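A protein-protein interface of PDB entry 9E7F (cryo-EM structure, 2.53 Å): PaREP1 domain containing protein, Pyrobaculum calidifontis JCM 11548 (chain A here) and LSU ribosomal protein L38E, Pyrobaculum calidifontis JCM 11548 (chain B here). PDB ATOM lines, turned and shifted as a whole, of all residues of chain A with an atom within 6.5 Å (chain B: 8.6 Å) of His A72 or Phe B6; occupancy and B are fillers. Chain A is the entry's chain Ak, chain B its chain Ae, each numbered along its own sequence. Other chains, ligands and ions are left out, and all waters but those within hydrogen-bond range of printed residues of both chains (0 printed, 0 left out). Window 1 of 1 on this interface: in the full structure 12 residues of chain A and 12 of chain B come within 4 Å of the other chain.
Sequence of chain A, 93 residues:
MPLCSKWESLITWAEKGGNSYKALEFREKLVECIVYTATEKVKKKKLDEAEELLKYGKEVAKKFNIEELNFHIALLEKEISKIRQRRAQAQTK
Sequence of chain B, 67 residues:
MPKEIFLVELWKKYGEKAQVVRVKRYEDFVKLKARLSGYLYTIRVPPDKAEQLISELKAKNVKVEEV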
ATOM      1  N   GLU A  28     -14.309   5.257 -17.079  1.00  0.00           N
ATOM      2  CA  GLU A  28     -14.809   6.564 -16.670  1.00  0.00           C
ATOM      3  C   GLU A  28     -15.364   7.344 -17.855  1.00  0.00           C
ATOM      4  O   GLU A  28     -16.398   8.010 -17.736  1.00  0.00           O
ATOM      5  CB  GLU A  28     -13.697   7.351 -15.986  1.00  0.00           C
ATOM      6  CG  GLU A  28     -13.974   8.830 -15.876  1.00  0.00           C
ATOM      7  CD  GLU A  28     -14.899   9.156 -14.732  1.00  0.00           C
ATOM      8  OE1 GLU A  28     -15.295   8.225 -14.003  1.00  0.00           O
ATOM      9  OE2 GLU A  28     -15.227  10.343 -14.554  1.00  0.00           O
ATOM     10  N   VAL A  31     -18.845   6.021 -18.787  1.00  0.00           N
ATOM     11  CA  VAL A  31     -19.890   6.523 -17.902  1.00  0.00           C
ATOM     12  C   VAL A  31     -20.146   8.000 -18.162  1.00  0.00           C
ATOM     13  O   VAL A  31     -21.286   8.467 -18.074  1.00  0.00           O
ATOM     14  CB  VAL A  31     -19.517   6.259 -16.436  1.00  0.00           C
ATOM     15  CG1 VAL A  31     -20.339   7.132 -15.515  1.00  0.00           C
ATOM     16  CG2 VAL A  31     -19.721   4.799 -16.109  1.00  0.00           C
ATOM     17  N   GLU A  32     -19.092   8.759 -18.469  1.00  0.00           N
ATOM     18  CA  GLU A  32     -19.261  10.172 -18.793  1.00  0.00           C
ATOM     19  C   GLU A  32     -20.076  10.362 -20.067  1.00  0.00           C
ATOM     20  O   GLU A  32     -20.908  11.272 -20.147  1.00  0.00           O
ATOM     21  CB  GLU A  32     -17.900  10.844 -18.944  1.00  0.00           C
ATOM     22  CG  GLU A  32     -17.215  11.170 -17.648  1.00  0.00           C
ATOM     23  CD  GLU A  32     -15.797  11.633 -17.870  1.00  0.00           C
ATOM     24  OE1 GLU A  32     -15.451  11.915 -19.036  1.00  0.00           O
ATOM     25  OE2 GLU A  32     -15.028  11.719 -16.890  1.00  0.00           O
ATOM     26  N   VAL A  35     -23.904   9.522 -19.057  1.00  0.00           N
ATOM     27  CA  VAL A  35     -24.563  10.420 -18.116  1.00  0.00           C
ATOM     28  C   VAL A  35     -24.635  11.835 -18.672  1.00  0.00           C
ATOM     29  O   VAL A  35     -25.642  12.528 -18.502  1.00  0.00           O
ATOM     30  CB  VAL A  35     -23.850  10.381 -16.754  1.00  0.00           C
ATOM     31  CG1 VAL A  35     -24.599  11.226 -15.747  1.00  0.00           C
ATOM     32  CG2 VAL A  35     -23.737   8.957 -16.270  1.00  0.00           C
ATOM     33  N   TYR A  36     -23.569  12.296 -19.327  1.00  0.00           N
ATOM     34  CA  TYR A  36     -23.554  13.658 -19.849  1.00  0.00           C
ATOM     35  C   TYR A  36     -24.563  13.831 -20.977  1.00  0.00           C
ATOM     36  O   TYR A  36     -25.323  14.804 -21.001  1.00  0.00           O
ATOM     37  CB  TYR A  36     -22.153  14.019 -20.336  1.00  0.00           C
ATOM     38  CG  TYR A  36     -21.174  14.376 -19.250  1.00  0.00           C
ATOM     39  CD1 TYR A  36     -21.608  14.834 -18.021  1.00  0.00           C
ATOM     40  CD2 TYR A  36     -19.811  14.258 -19.461  1.00  0.00           C
ATOM     41  CE1 TYR A  36     -20.712  15.162 -17.032  1.00  0.00           C
ATOM     42  CE2 TYR A  36     -18.911  14.582 -18.479  1.00  0.00           C
ATOM     43  CZ  TYR A  36     -19.366  15.035 -17.268  1.00  0.00           C
ATOM     44  OH  TYR A  36     -18.470  15.363 -16.284  1.00  0.00           O
ATOM     45  N   THR A  39     -28.044  13.480 -19.540  1.00  0.00           N
ATOM     46  CA  THR A  39     -28.418  14.602 -18.687  1.00  0.00           C
ATOM     47  C   THR A  39     -28.694  15.854 -19.503  1.00  0.00           C
ATOM     48  O   THR A  39     -29.488  16.703 -19.087  1.00  0.00           O
ATOM     49  CB  THR A  39     -27.327  14.872 -17.653  1.00  0.00           C
ATOM     50  OG1 THR A  39     -27.047  13.667 -16.937  1.00  0.00           O
ATOM     51  CG2 THR A  39     -27.776  15.928 -16.671  1.00  0.00           C
ATOM     52  N   LEU A  54     -30.725   5.978 -21.667  1.00  0.00           N
ATOM     53  CA  LEU A  54     -30.740   5.416 -20.318  1.00  0.00           C
ATOM     54  C   LEU A  54     -30.915   3.904 -20.342  1.00  0.00           C
ATOM     55  O   LEU A  54     -30.320   3.195 -19.525  1.00  0.00           O
ATOM     56  CB  LEU A  54     -31.847   6.064 -19.489  1.00  0.00           C
ATOM     57  CG  LEU A  54     -31.697   7.560 -19.234  1.00  0.00           C
ATOM     58  CD1 LEU A  54     -32.945   8.120 -18.573  1.00  0.00           C
ATOM     59  CD2 LEU A  54     -30.470   7.827 -18.385  1.00  0.00           C
ATOM     60  N   GLU A  67     -21.642   0.389 -10.930  1.00  0.00           N
ATOM     61  CA  GLU A  67     -22.761   0.788 -10.081  1.00  0.00           C
ATOM     62  C   GLU A  67     -23.075   2.261 -10.290  1.00  0.00           C
ATOM     63  O   GLU A  67     -24.237   2.671 -10.188  1.00  0.00           O
ATOM     64  CB  GLU A  67     -22.443   0.428  -8.615  1.00  0.00           C
ATOM     65  CG  GLU A  67     -23.508   0.623  -7.476  1.00  0.00           C
ATOM     66  CD  GLU A  67     -24.041   2.021  -7.124  1.00  0.00           C
ATOM     67  OE1 GLU A  67     -24.915   2.074  -6.236  1.00  0.00           O
ATOM     68  OE2 GLU A  67     -23.509   3.066  -7.534  1.00  0.00           O
ATOM     69  N   GLU A  68     -22.051   3.070 -10.584  1.00  0.00           N
ATOM     70  CA  GLU A  68     -22.235   4.513 -10.704  1.00  0.00           C
ATOM     71  C   GLU A  68     -23.143   4.870 -11.872  1.00  0.00           C
ATOM     72  O   GLU A  68     -23.830   5.894 -11.828  1.00  0.00           O
ATOM     73  CB  GLU A  68     -20.883   5.201 -10.845  1.00  0.00           C
ATOM     74  CG  GLU A  68     -20.000   5.017  -9.638  1.00  0.00           C
ATOM     75  CD  GLU A  68     -19.067   3.832  -9.774  1.00  0.00           C
ATOM     76  OE1 GLU A  68     -19.416   2.879 -10.499  1.00  0.00           O
ATOM     77  OE2 GLU A  68     -17.990   3.846  -9.146  1.00  0.00           O
ATOM     78  N   LEU A  69     -23.160   4.047 -12.921  1.00  0.00           N
ATOM     79  CA  LEU A  69     -24.171   4.216 -13.957  1.00  0.00           C
ATOM     80  C   LEU A  69     -25.563   3.969 -13.396  1.00  0.00           C
ATOM     81  O   LEU A  69     -26.498   4.725 -13.681  1.00  0.00           O
ATOM     82  CB  LEU A  69     -23.894   3.275 -15.123  1.00  0.00           C
ATOM     83  CG  LEU A  69     -23.363   3.926 -16.394  1.00  0.00           C
ATOM     84  CD1 LEU A  69     -22.926   2.862 -17.381  1.00  0.00           C
ATOM     85  CD2 LEU A  69     -24.400   4.840 -17.009  1.00  0.00           C
ATOM     86  N   ASN A  70     -25.712   2.921 -12.583  1.00  0.00           N
ATOM     87  CA  ASN A  70     -27.011   2.610 -11.997  1.00  0.00           C
ATOM     88  C   ASN A  70     -27.472   3.710 -11.050  1.00  0.00           C
ATOM     89  O   ASN A  70     -28.652   4.074 -11.043  1.00  0.00           O
ATOM     90  CB  ASN A  70     -26.951   1.271 -11.266  1.00  0.00           C
ATOM     91  CG  ASN A  70     -26.547   0.133 -12.170  1.00  0.00           C
ATOM     92  OD1 ASN A  70     -25.566  -0.563 -11.912  1.00  0.00           O
ATOM     93  ND2 ASN A  70     -27.305  -0.069 -13.238  1.00  0.00           N
ATOM     94  N   PHE A  71     -26.556   4.248 -10.241  1.00  0.00           N
ATOM     95  CA  PHE A  71     -26.916   5.343  -9.345  1.00  0.00           C
ATOM     96  C   PHE A  71     -27.302   6.594 -10.125  1.00  0.00           C
ATOM     97  O   PHE A  71     -28.289   7.257  -9.795  1.00  0.00           O
ATOM     98  CB  PHE A  71     -25.760   5.637  -8.389  1.00  0.00           C
ATOM     99  CG  PHE A  71     -25.883   6.950  -7.669  1.00  0.00           C
ATOM    100  CD1 PHE A  71     -26.965   7.212  -6.849  1.00  0.00           C
ATOM    101  CD2 PHE A  71     -24.911   7.922  -7.812  1.00  0.00           C
ATOM    102  CE1 PHE A  71     -27.074   8.418  -6.191  1.00  0.00           C
ATOM    103  CE2 PHE A  71     -25.019   9.131  -7.156  1.00  0.00           C
ATOM    104  CZ  PHE A  71     -26.099   9.378  -6.345  1.00  0.00           C
ATOM    105  N   HIS A  72     -26.540   6.934 -11.161  1.00  0.00           N
ATOM    106  CA  HIS A  72     -26.842   8.143 -11.913  1.00  0.00           C
ATOM    107  C   HIS A  72     -28.041   7.962 -12.830  1.00  0.00           C
ATOM    108  O   HIS A  72     -28.761   8.929 -13.097  1.00  0.00           O
ATOM    109  CB  HIS A  72     -25.619   8.581 -12.712  1.00  0.00           C
ATOM    110  CG  HIS A  72     -24.612   9.328 -11.901  1.00  0.00           C
ATOM    111  ND1 HIS A  72     -24.817  10.620 -11.471  1.00  0.00           N
ATOM    112  CD2 HIS A  72     -23.397   8.962 -11.432  1.00  0.00           C
ATOM    113  CE1 HIS A  72     -23.768  11.021 -10.774  1.00  0.00           C
ATOM    114  NE2 HIS A  72     -22.893  10.033 -10.735  1.00  0.00           N
ATOM    115  N   ILE A  73     -28.262   6.748 -13.332  1.00  0.00           N
ATOM    116  CA  ILE A  73     -29.441   6.497 -14.151  1.00  0.00           C
ATOM    117  C   ILE A  73     -30.705   6.611 -13.310  1.00  0.00           C
ATOM    118  O   ILE A  73     -31.745   7.074 -13.790  1.00  0.00           O
ATOM    119  CB  ILE A  73     -29.335   5.126 -14.838  1.00  0.00           C
ATOM    120  CG1 ILE A  73     -28.339   5.190 -15.994  1.00  0.00           C
ATOM    121  CG2 ILE A  73     -30.691   4.680 -15.345  1.00  0.00           C
ATOM    122  CD1 ILE A  73     -27.808   3.840 -16.408  1.00  0.00           C
ATOM    123  N   ALA A  74     -30.636   6.191 -12.045  1.00  0.00           N
ATOM    124  CA  ALA A  74     -31.786   6.329 -11.159  1.00  0.00           C
ATOM    125  C   ALA A  74     -32.115   7.794 -10.904  1.00  0.00           C
ATOM    126  O   ALA A  74     -33.290   8.164 -10.804  1.00  0.00           O
ATOM    127  CB  ALA A  74     -31.524   5.601  -9.844  1.00  0.00           C
ATOM    128  N   LEU A  75     -31.092   8.640 -10.786  1.00  0.00           N
ATOM    129  CA  LEU A  75     -31.336  10.070 -10.631  1.00  0.00           C
ATOM    130  C   LEU A  75     -31.993  10.658 -11.875  1.00  0.00           C
ATOM    131  O   LEU A  75     -32.870  11.521 -11.773  1.00  0.00           O
ATOM    132  CB  LEU A  75     -30.028  10.799 -10.325  1.00  0.00           C
ATOM    133  CG  LEU A  75     -29.386  10.606  -8.953  1.00  0.00           C
ATOM    134  CD1 LEU A  75     -28.056  11.330  -8.879  1.00  0.00           C
ATOM    135  CD2 LEU A  75     -30.308  11.086  -7.856  1.00  0.00           C
ATOM    136  N   LEU A  76     -31.576  10.212 -13.062  1.00  0.00           N
ATOM    137  CA  LEU A  76     -32.123  10.774 -14.293  1.00  0.00           C
ATOM    138  C   LEU A  76     -33.545  10.293 -14.546  1.00  0.00           C
ATOM    139  O   LEU A  76     -34.368  11.041 -15.085  1.00  0.00           O
ATOM    140  CB  LEU A  76     -31.224  10.432 -15.477  1.00  0.00           C
ATOM    141  CG  LEU A  76     -30.045  11.377 -15.702  1.00  0.00           C
ATOM    142  CD1 LEU A  76     -29.362  11.079 -17.019  1.00  0.00           C
ATOM    143  CD2 LEU A  76     -30.514  12.813 -15.660  1.00  0.00           C
ATOM    144  N   GLU A  77     -33.852   9.045 -14.184  1.00  0.00           N
ATOM    145  CA  GLU A  77     -35.212   8.545 -14.358  1.00  0.00           C
ATOM    146  C   GLU A  77     -36.183   9.262 -13.435  1.00  0.00           C
ATOM    147  O   GLU A  77     -37.340   9.494 -13.801  1.00  0.00           O
ATOM    148  CB  GLU A  77     -35.264   7.040 -14.113  1.00  0.00           C
ATOM    149  CG  GLU A  77     -34.381   6.232 -15.037  1.00  0.00           C
ATOM    150  CD  GLU A  77     -35.169   5.488 -16.092  1.00  0.00           C
ATOM    151  OE1 GLU A  77     -35.836   4.492 -15.742  1.00  0.00           O
ATOM    152  OE2 GLU A  77     -35.117   5.892 -17.275  1.00  0.00           O
ATOM    153  N   LYS B   3     -12.441  19.341 -12.191  1.00  0.00           N
ATOM    154  CA  LYS B   3     -12.776  18.159 -12.963  1.00  0.00           C
ATOM    155  C   LYS B   3     -13.756  17.296 -12.186  1.00  0.00           C
ATOM    156  O   LYS B   3     -13.760  17.287 -10.954  1.00  0.00           O
ATOM    157  CB  LYS B   3     -11.534  17.338 -13.299  1.00  0.00           C
ATOM    158  CG  LYS B   3     -10.530  18.051 -14.174  1.00  0.00           C
ATOM    159  CD  LYS B   3      -9.177  17.389 -14.058  1.00  0.00           C
ATOM    160  CE  LYS B   3      -8.565  17.138 -15.414  1.00  0.00           C
ATOM    161  NZ  LYS B   3      -7.971  18.371 -15.972  1.00  0.00           N
ATOM    162  N   GLU B   4     -14.582  16.563 -12.923  1.00  0.00           N
ATOM    163  CA  GLU B   4     -15.590  15.686 -12.352  1.00  0.00           C
ATOM    164  C   GLU B   4     -15.260  14.244 -12.701  1.00  0.00           C
ATOM    165  O   GLU B   4     -14.884  13.950 -13.839  1.00  0.00           O
ATOM    166  CB  GLU B   4     -16.982  16.049 -12.866  1.00  0.00           C
ATOM    167  CG  GLU B   4     -18.078  15.156 -12.343  1.00  0.00           C
ATOM    168  CD  GLU B   4     -19.440  15.578 -12.836  1.00  0.00           C
ATOM    169  OE1 GLU B   4     -19.502  16.424 -13.747  1.00  0.00           O
ATOM    170  OE2 GLU B   4     -20.450  15.066 -12.313  1.00  0.00           O
ATOM    171  N   ILE B   5     -15.398  13.353 -11.727  1.00  0.00           N
ATOM    172  CA  ILE B   5     -15.110  11.938 -11.911  1.00  0.00           C
ATOM    173  C   ILE B   5     -16.290  11.124 -11.408  1.00  0.00           C
ATOM    174  O   ILE B   5     -16.907  11.451 -10.392  1.00  0.00           O
ATOM    175  CB  ILE B   5     -13.813  11.527 -11.194  1.00  0.00           C
ATOM    176  CG1 ILE B   5     -12.665  12.404 -11.675  1.00  0.00           C
ATOM    177  CG2 ILE B   5     -13.502  10.069 -11.452  1.00  0.00           C
ATOM    178  CD1 ILE B   5     -11.346  12.007 -11.110  1.00  0.00           C
ATOM    179  N   PHE B   6     -16.607  10.053 -12.134  1.00  0.00           N
ATOM    180  CA  PHE B   6     -17.811   9.286 -11.871  1.00  0.00           C
ATOM    181  C   PHE B   6     -17.570   7.952 -11.188  1.00  0.00           C
ATOM    182  O   PHE B   6     -18.489   7.439 -10.549  1.00  0.00           O
ATOM    183  CB  PHE B   6     -18.575   9.041 -13.175  1.00  0.00           C
ATOM    184  CG  PHE B   6     -19.415  10.195 -13.593  1.00  0.00           C
ATOM    185  CD1 PHE B   6     -20.728  10.290 -13.186  1.00  0.00           C
ATOM    186  CD2 PHE B   6     -18.886  11.198 -14.376  1.00  0.00           C
ATOM    187  CE1 PHE B   6     -21.503  11.355 -13.564  1.00  0.00           C
ATOM    188  CE2 PHE B   6     -19.656  12.264 -14.758  1.00  0.00           C
ATOM    189  CZ  PHE B   6     -20.967  12.344 -14.352  1.00  0.00           C
ATOM    190  N   LEU B   7     -16.379   7.381 -11.305  1.00  0.00           N
ATOM    191  CA  LEU B   7     -16.051   6.129 -10.638  1.00  0.00           C
ATOM    192  C   LEU B   7     -15.321   6.426  -9.337  1.00  0.00           C
ATOM    193  O   LEU B   7     -14.333   7.164  -9.333  1.00  0.00           O
ATOM    194  CB  LEU B   7     -15.192   5.244 -11.535  1.00  0.00           C
ATOM    195  CG  LEU B   7     -15.737   5.054 -12.945  1.00  0.00           C
ATOM    196  CD1 LEU B   7     -14.959   3.970 -13.652  1.00  0.00           C
ATOM    197  CD2 LEU B   7     -17.205   4.720 -12.888  1.00  0.00           C
ATOM    198  N   VAL B   8     -15.807   5.848  -8.238  1.00  0.00           N
ATOM    199  CA  VAL B   8     -15.212   6.128  -6.935  1.00  0.00           C
ATOM    200  C   VAL B   8     -13.803   5.560  -6.846  1.00  0.00           C
ATOM    201  O   VAL B   8     -12.959   6.098  -6.124  1.00  0.00           O
ATOM    202  CB  VAL B   8     -16.117   5.606  -5.799  1.00  0.00           C
ATOM    203  CG1 VAL B   8     -15.641   4.274  -5.284  1.00  0.00           C
ATOM    204  CG2 VAL B   8     -16.169   6.604  -4.675  1.00  0.00           C
ATOM    205  N   GLU B   9     -13.521   4.481  -7.581  1.00  0.00           N
ATOM    206  CA  GLU B   9     -12.180   3.905  -7.582  1.00  0.00           C
ATOM    207  C   GLU B   9     -11.169   4.872  -8.181  1.00  0.00           C
ATOM    208  O   GLU B   9     -10.059   5.031  -7.663  1.00  0.00           O
ATOM    209  CB  GLU B   9     -12.178   2.587  -8.353  1.00  0.00           C
ATOM    210  CG  GLU B   9     -12.730   1.412  -7.575  1.00  0.00           C
ATOM    211  CD  GLU B   9     -14.246   1.355  -7.598  1.00  0.00           C
ATOM    212  OE1 GLU B   9     -14.881   2.427  -7.549  1.00  0.00           O
ATOM    213  OE2 GLU B   9     -14.802   0.239  -7.667  1.00  0.00           O
ATOM    214  N   LEU B  10     -11.537   5.520  -9.284  1.00  0.00           N
ATOM    215  CA  LEU B  10     -10.663   6.522  -9.876  1.00  0.00           C
ATOM    216  C   LEU B  10     -10.543   7.748  -8.981  1.00  0.00           C
ATOM    217  O   LEU B  10      -9.451   8.300  -8.818  1.00  0.00           O
ATOM    218  CB  LEU B  10     -11.186   6.898 -11.261  1.00  0.00           C
ATOM    219  CG  LEU B  10     -10.476   7.968 -12.087  1.00  0.00           C
ATOM    220  CD1 LEU B  10      -9.051   7.570 -12.406  1.00  0.00           C
ATOM    221  CD2 LEU B  10     -11.259   8.214 -13.365  1.00  0.00           C
ATOM    222  N   TRP B  11     -11.653   8.181  -8.379  1.00  0.00           N
ATOM    223  CA  TRP B  11     -11.625   9.374  -7.541  1.00  0.00           C
ATOM    224  C   TRP B  11     -10.849   9.146  -6.252  1.00  0.00           C
ATOM    225  O   TRP B  11     -10.298  10.096  -5.689  1.00  0.00           O
ATOM    226  CB  TRP B  11     -13.049   9.831  -7.226  1.00  0.00           C
ATOM    227  CG  TRP B  11     -13.115  11.115  -6.460  1.00  0.00           C
ATOM    228  CD1 TRP B  11     -13.135  12.375  -6.976  1.00  0.00           C
ATOM    229  CD2 TRP B  11     -13.173  11.265  -5.041  1.00  0.00           C
ATOM    230  NE1 TRP B  11     -13.198  13.300  -5.968  1.00  0.00           N
ATOM    231  CE2 TRP B  11     -13.222  12.643  -4.769  1.00  0.00           C
ATOM    232  CE3 TRP B  11     -13.182  10.368  -3.973  1.00  0.00           C
ATOM    233  CZ2 TRP B  11     -13.283  13.143  -3.475  1.00  0.00           C
ATOM    234  CZ3 TRP B  11     -13.238  10.865  -2.694  1.00  0.00           C
ATOM    235  CH2 TRP B  11     -13.288  12.239  -2.453  1.00  0.00           C
ATOM    236  N   ASP B  28     -30.339  13.502  -2.399  1.00  0.00           N
ATOM    237  CA  ASP B  28     -30.100  12.283  -3.158  1.00  0.00           C
ATOM    238  C   ASP B  28     -28.626  11.975  -3.346  1.00  0.00           C
ATOM    239  O   ASP B  28     -28.294  10.866  -3.774  1.00  0.00           O
ATOM    240  CB  ASP B  28     -30.763  12.369  -4.538  1.00  0.00           C
ATOM    241  CG  ASP B  28     -32.094  13.068  -4.499  1.00  0.00           C
ATOM    242  OD1 ASP B  28     -32.100  14.313  -4.528  1.00  0.00           O
ATOM    243  OD2 ASP B  28     -33.130  12.375  -4.431  1.00  0.00           O
ATOM    244  N   PHE B  29     -27.741  12.914  -3.044  1.00  0.00           N
ATOM    245  CA  PHE B  29     -26.329  12.708  -3.317  1.00  0.00           C
ATOM    246  C   PHE B  29     -25.518  13.645  -2.441  1.00  0.00           C
ATOM    247  O   PHE B  29     -26.042  14.589  -1.847  1.00  0.00           O
ATOM    248  CB  PHE B  29     -26.014  12.913  -4.804  1.00  0.00           C
ATOM    249  CG  PHE B  29     -26.236  14.314  -5.290  1.00  0.00           C
ATOM    250  CD1 PHE B  29     -27.499  14.749  -5.651  1.00  0.00           C
ATOM    251  CD2 PHE B  29     -25.176  15.194  -5.410  1.00  0.00           C
ATOM    252  CE1 PHE B  29     -27.701  16.035  -6.102  1.00  0.00           C
ATOM    253  CE2 PHE B  29     -25.375  16.478  -5.863  1.00  0.00           C
ATOM    254  CZ  PHE B  29     -26.636  16.899  -6.210  1.00  0.00           C
ATOM    255  N   VAL B  30     -24.227  13.359  -2.363  1.00  0.00           N
ATOM    256  CA  VAL B  30     -23.264  14.204  -1.675  1.00  0.00           C
ATOM    257  C   VAL B  30     -22.139  14.509  -2.646  1.00  0.00           C
ATOM    258  O   VAL B  30     -21.680  13.625  -3.375  1.00  0.00           O
ATOM    259  CB  VAL B  30     -22.717  13.533  -0.402  1.00  0.00           C
ATOM    260  CG1 VAL B  30     -21.582  14.350   0.171  1.00  0.00           C
ATOM    261  CG2 VAL B  30     -23.819  13.367   0.618  1.00  0.00           C
ATOM    262  N   THR B  42     -14.110  16.557  -8.150  1.00  0.00           N
ATOM    263  CA  THR B  42     -15.437  16.444  -7.565  1.00  0.00           C
ATOM    264  C   THR B  42     -16.101  15.155  -8.024  1.00  0.00           C
ATOM    265  O   THR B  42     -16.022  14.792  -9.198  1.00  0.00           O
ATOM    266  CB  THR B  42     -16.305  17.646  -7.954  1.00  0.00           C
ATOM    267  OG1 THR B  42     -15.833  18.815  -7.276  1.00  0.00           O
ATOM    268  CG2 THR B  42     -17.761  17.413  -7.595  1.00  0.00           C
ATOM    269  N   ILE B  43     -16.750  14.464  -7.091  1.00  0.00           N
ATOM    270  CA  ILE B  43     -17.543  13.280  -7.394  1.00  0.00           C
ATOM    271  C   ILE B  43     -18.885  13.405  -6.690  1.00  0.00           C
ATOM    272  O   ILE B  43     -18.962  13.895  -5.560  1.00  0.00           O
ATOM    273  CB  ILE B  43     -16.828  11.983  -6.972  1.00  0.00           C
ATOM    274  CG1 ILE B  43     -17.598  10.764  -7.474  1.00  0.00           C
ATOM    275  CG2 ILE B  43     -16.693  11.913  -5.474  1.00  0.00           C
ATOM    276  CD1 ILE B  43     -16.745   9.540  -7.647  1.00  0.00           C
ATOM    277  N   ARG B  44     -19.944  12.977  -7.364  1.00  0.00           N
ATOM    278  CA  ARG B  44     -21.274  12.906  -6.775  1.00  0.00           C
ATOM    279  C   ARG B  44     -21.588  11.450  -6.465  1.00  0.00           C
ATOM    280  O   ARG B  44     -21.607  10.611  -7.369  1.00  0.00           O
ATOM    281  CB  ARG B  44     -22.328  13.490  -7.712  1.00  0.00           C
ATOM    282  CG  ARG B  44     -22.508  14.982  -7.581  1.00  0.00           C
ATOM    283  CD  ARG B  44     -22.389  15.654  -8.922  1.00  0.00           C
ATOM    284  NE  ARG B  44     -23.627  15.573  -9.682  1.00  0.00           N
ATOM    285  CZ  ARG B  44     -23.695  15.199 -10.951  1.00  0.00           C
ATOM    286  NH1 ARG B  44     -22.615  14.843 -11.622  1.00  0.00           N
ATOM    287  NH2 ARG B  44     -24.876  15.188 -11.563  1.00  0.00           N
ATOM    288  N   VAL B  45     -21.849  11.160  -5.196  1.00  0.00           N
ATOM    289  CA  VAL B  45     -22.039   9.785  -4.742  1.00  0.00           C
ATOM    290  C   VAL B  45     -23.361   9.702  -3.994  1.00  0.00           C
ATOM    291  O   VAL B  45     -23.911  10.727  -3.562  1.00  0.00           O
ATOM    292  CB  VAL B  45     -20.871   9.312  -3.847  1.00  0.00           C
ATOM    293  CG1 VAL B  45     -19.577   9.308  -4.634  1.00  0.00           C
ATOM    294  CG2 VAL B  45     -20.752  10.198  -2.625  1.00  0.00           C
ATOM    295  N   PRO B  46     -23.908   8.494  -3.842  1.00  0.00           N
ATOM    296  CA  PRO B  46     -25.107   8.339  -3.024  1.00  0.00           C
ATOM    297  C   PRO B  46     -24.799   8.680  -1.583  1.00  0.00           C
ATOM    298  O   PRO B  46     -23.629   8.651  -1.162  1.00  0.00           O
ATOM    299  CB  PRO B  46     -25.461   6.849  -3.185  1.00  0.00           C
ATOM    300  CG  PRO B  46     -24.564   6.310  -4.226  1.00  0.00           C
ATOM    301  CD  PRO B  46     -23.398   7.214  -4.351  1.00  0.00           C
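N of Leu B7 is in hydrogen-bond range of OE1 of Glu A28, 3.0 Å away.
OE1 of Glu B4 lies within hydrogen-bond range of OH of Tyr A36.
The backbone NH (N) of Phe B6 lies within hydrogen-bond range of the side-chain carboxylate (OE2) of Glu A28 (2.8 Å).
The side-chain carboxylate of Glu A68 lies within hydrogen-bond range of the backbone NH of Val B8 (3.1 Å).
The backbone carbonyl oxygen of Val B45 lies within hydrogen-bond range of the backbone NH of Val B30.
N of Ile B5 is in hydrogen-bond range of O of Thr B42 (3.0 Å).
The side-chain carboxylate of Glu A32 lies close to the side-chain carboxylate of Glu A28, at 2.7 Å.
Glu A28 touches Glu B4 (OE2 to O, 3.7 Å).
Glu A28 touches Ile B5 (OE2 to CA, 3.1 Å).
O of Glu B4 touches OE2 of Glu A32, at 3.8 Å.
Leu B7 touches Glu A68 (CA to OE2, 3.3 Å).
Phe B29 touches Phe A71.
O of Arg B44 touches CE2 of Phe A71 (3.7 Å).
Pro B46 touches Phe A71 (N to CZ, 3.4 Å).
NE2 of His A72 touches CD1 of Phe B6, at 3.3 Å.
His A72 touches Arg B44 (NE2 to O, 3.6 Å).
Asp B28 touches Leu A75.
Of chain B, only Phe B6 and Arg B44 come within 4 Å of His A72.
Of chain A, only Glu A28, Val A31, Glu A32, Val A35, Tyr A36, Glu A68 and His A72 come within 4 Å of Phe B6.
Printed residues of chain A within 4 Å of Phe B29: Phe A71 (3.9 Å).
Of the printed residues of chain B, Leu A75 touches Asp B28.
Printed residues of chain A within 4 Å of Val B8: Glu A68 (3.1 Å).
Of the printed residues of chain A, Pro B46 touches Phe A71 (3.4 Å).
Of the printed residues of chain B, Tyr A36 touches Glu B4 and Phe B6.
Leu A69 touches none of the printed residues of chain B.
The nearest printed residue of chain A that does not touch Glu B9 is Glu A67 (7.6 Å).
Hydrophobic or aromatic side chains of chain B that line the printed part of chain A: Ile B5, Phe B6, Leu B7, Leu B10, Phe B29 and Pro B46.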
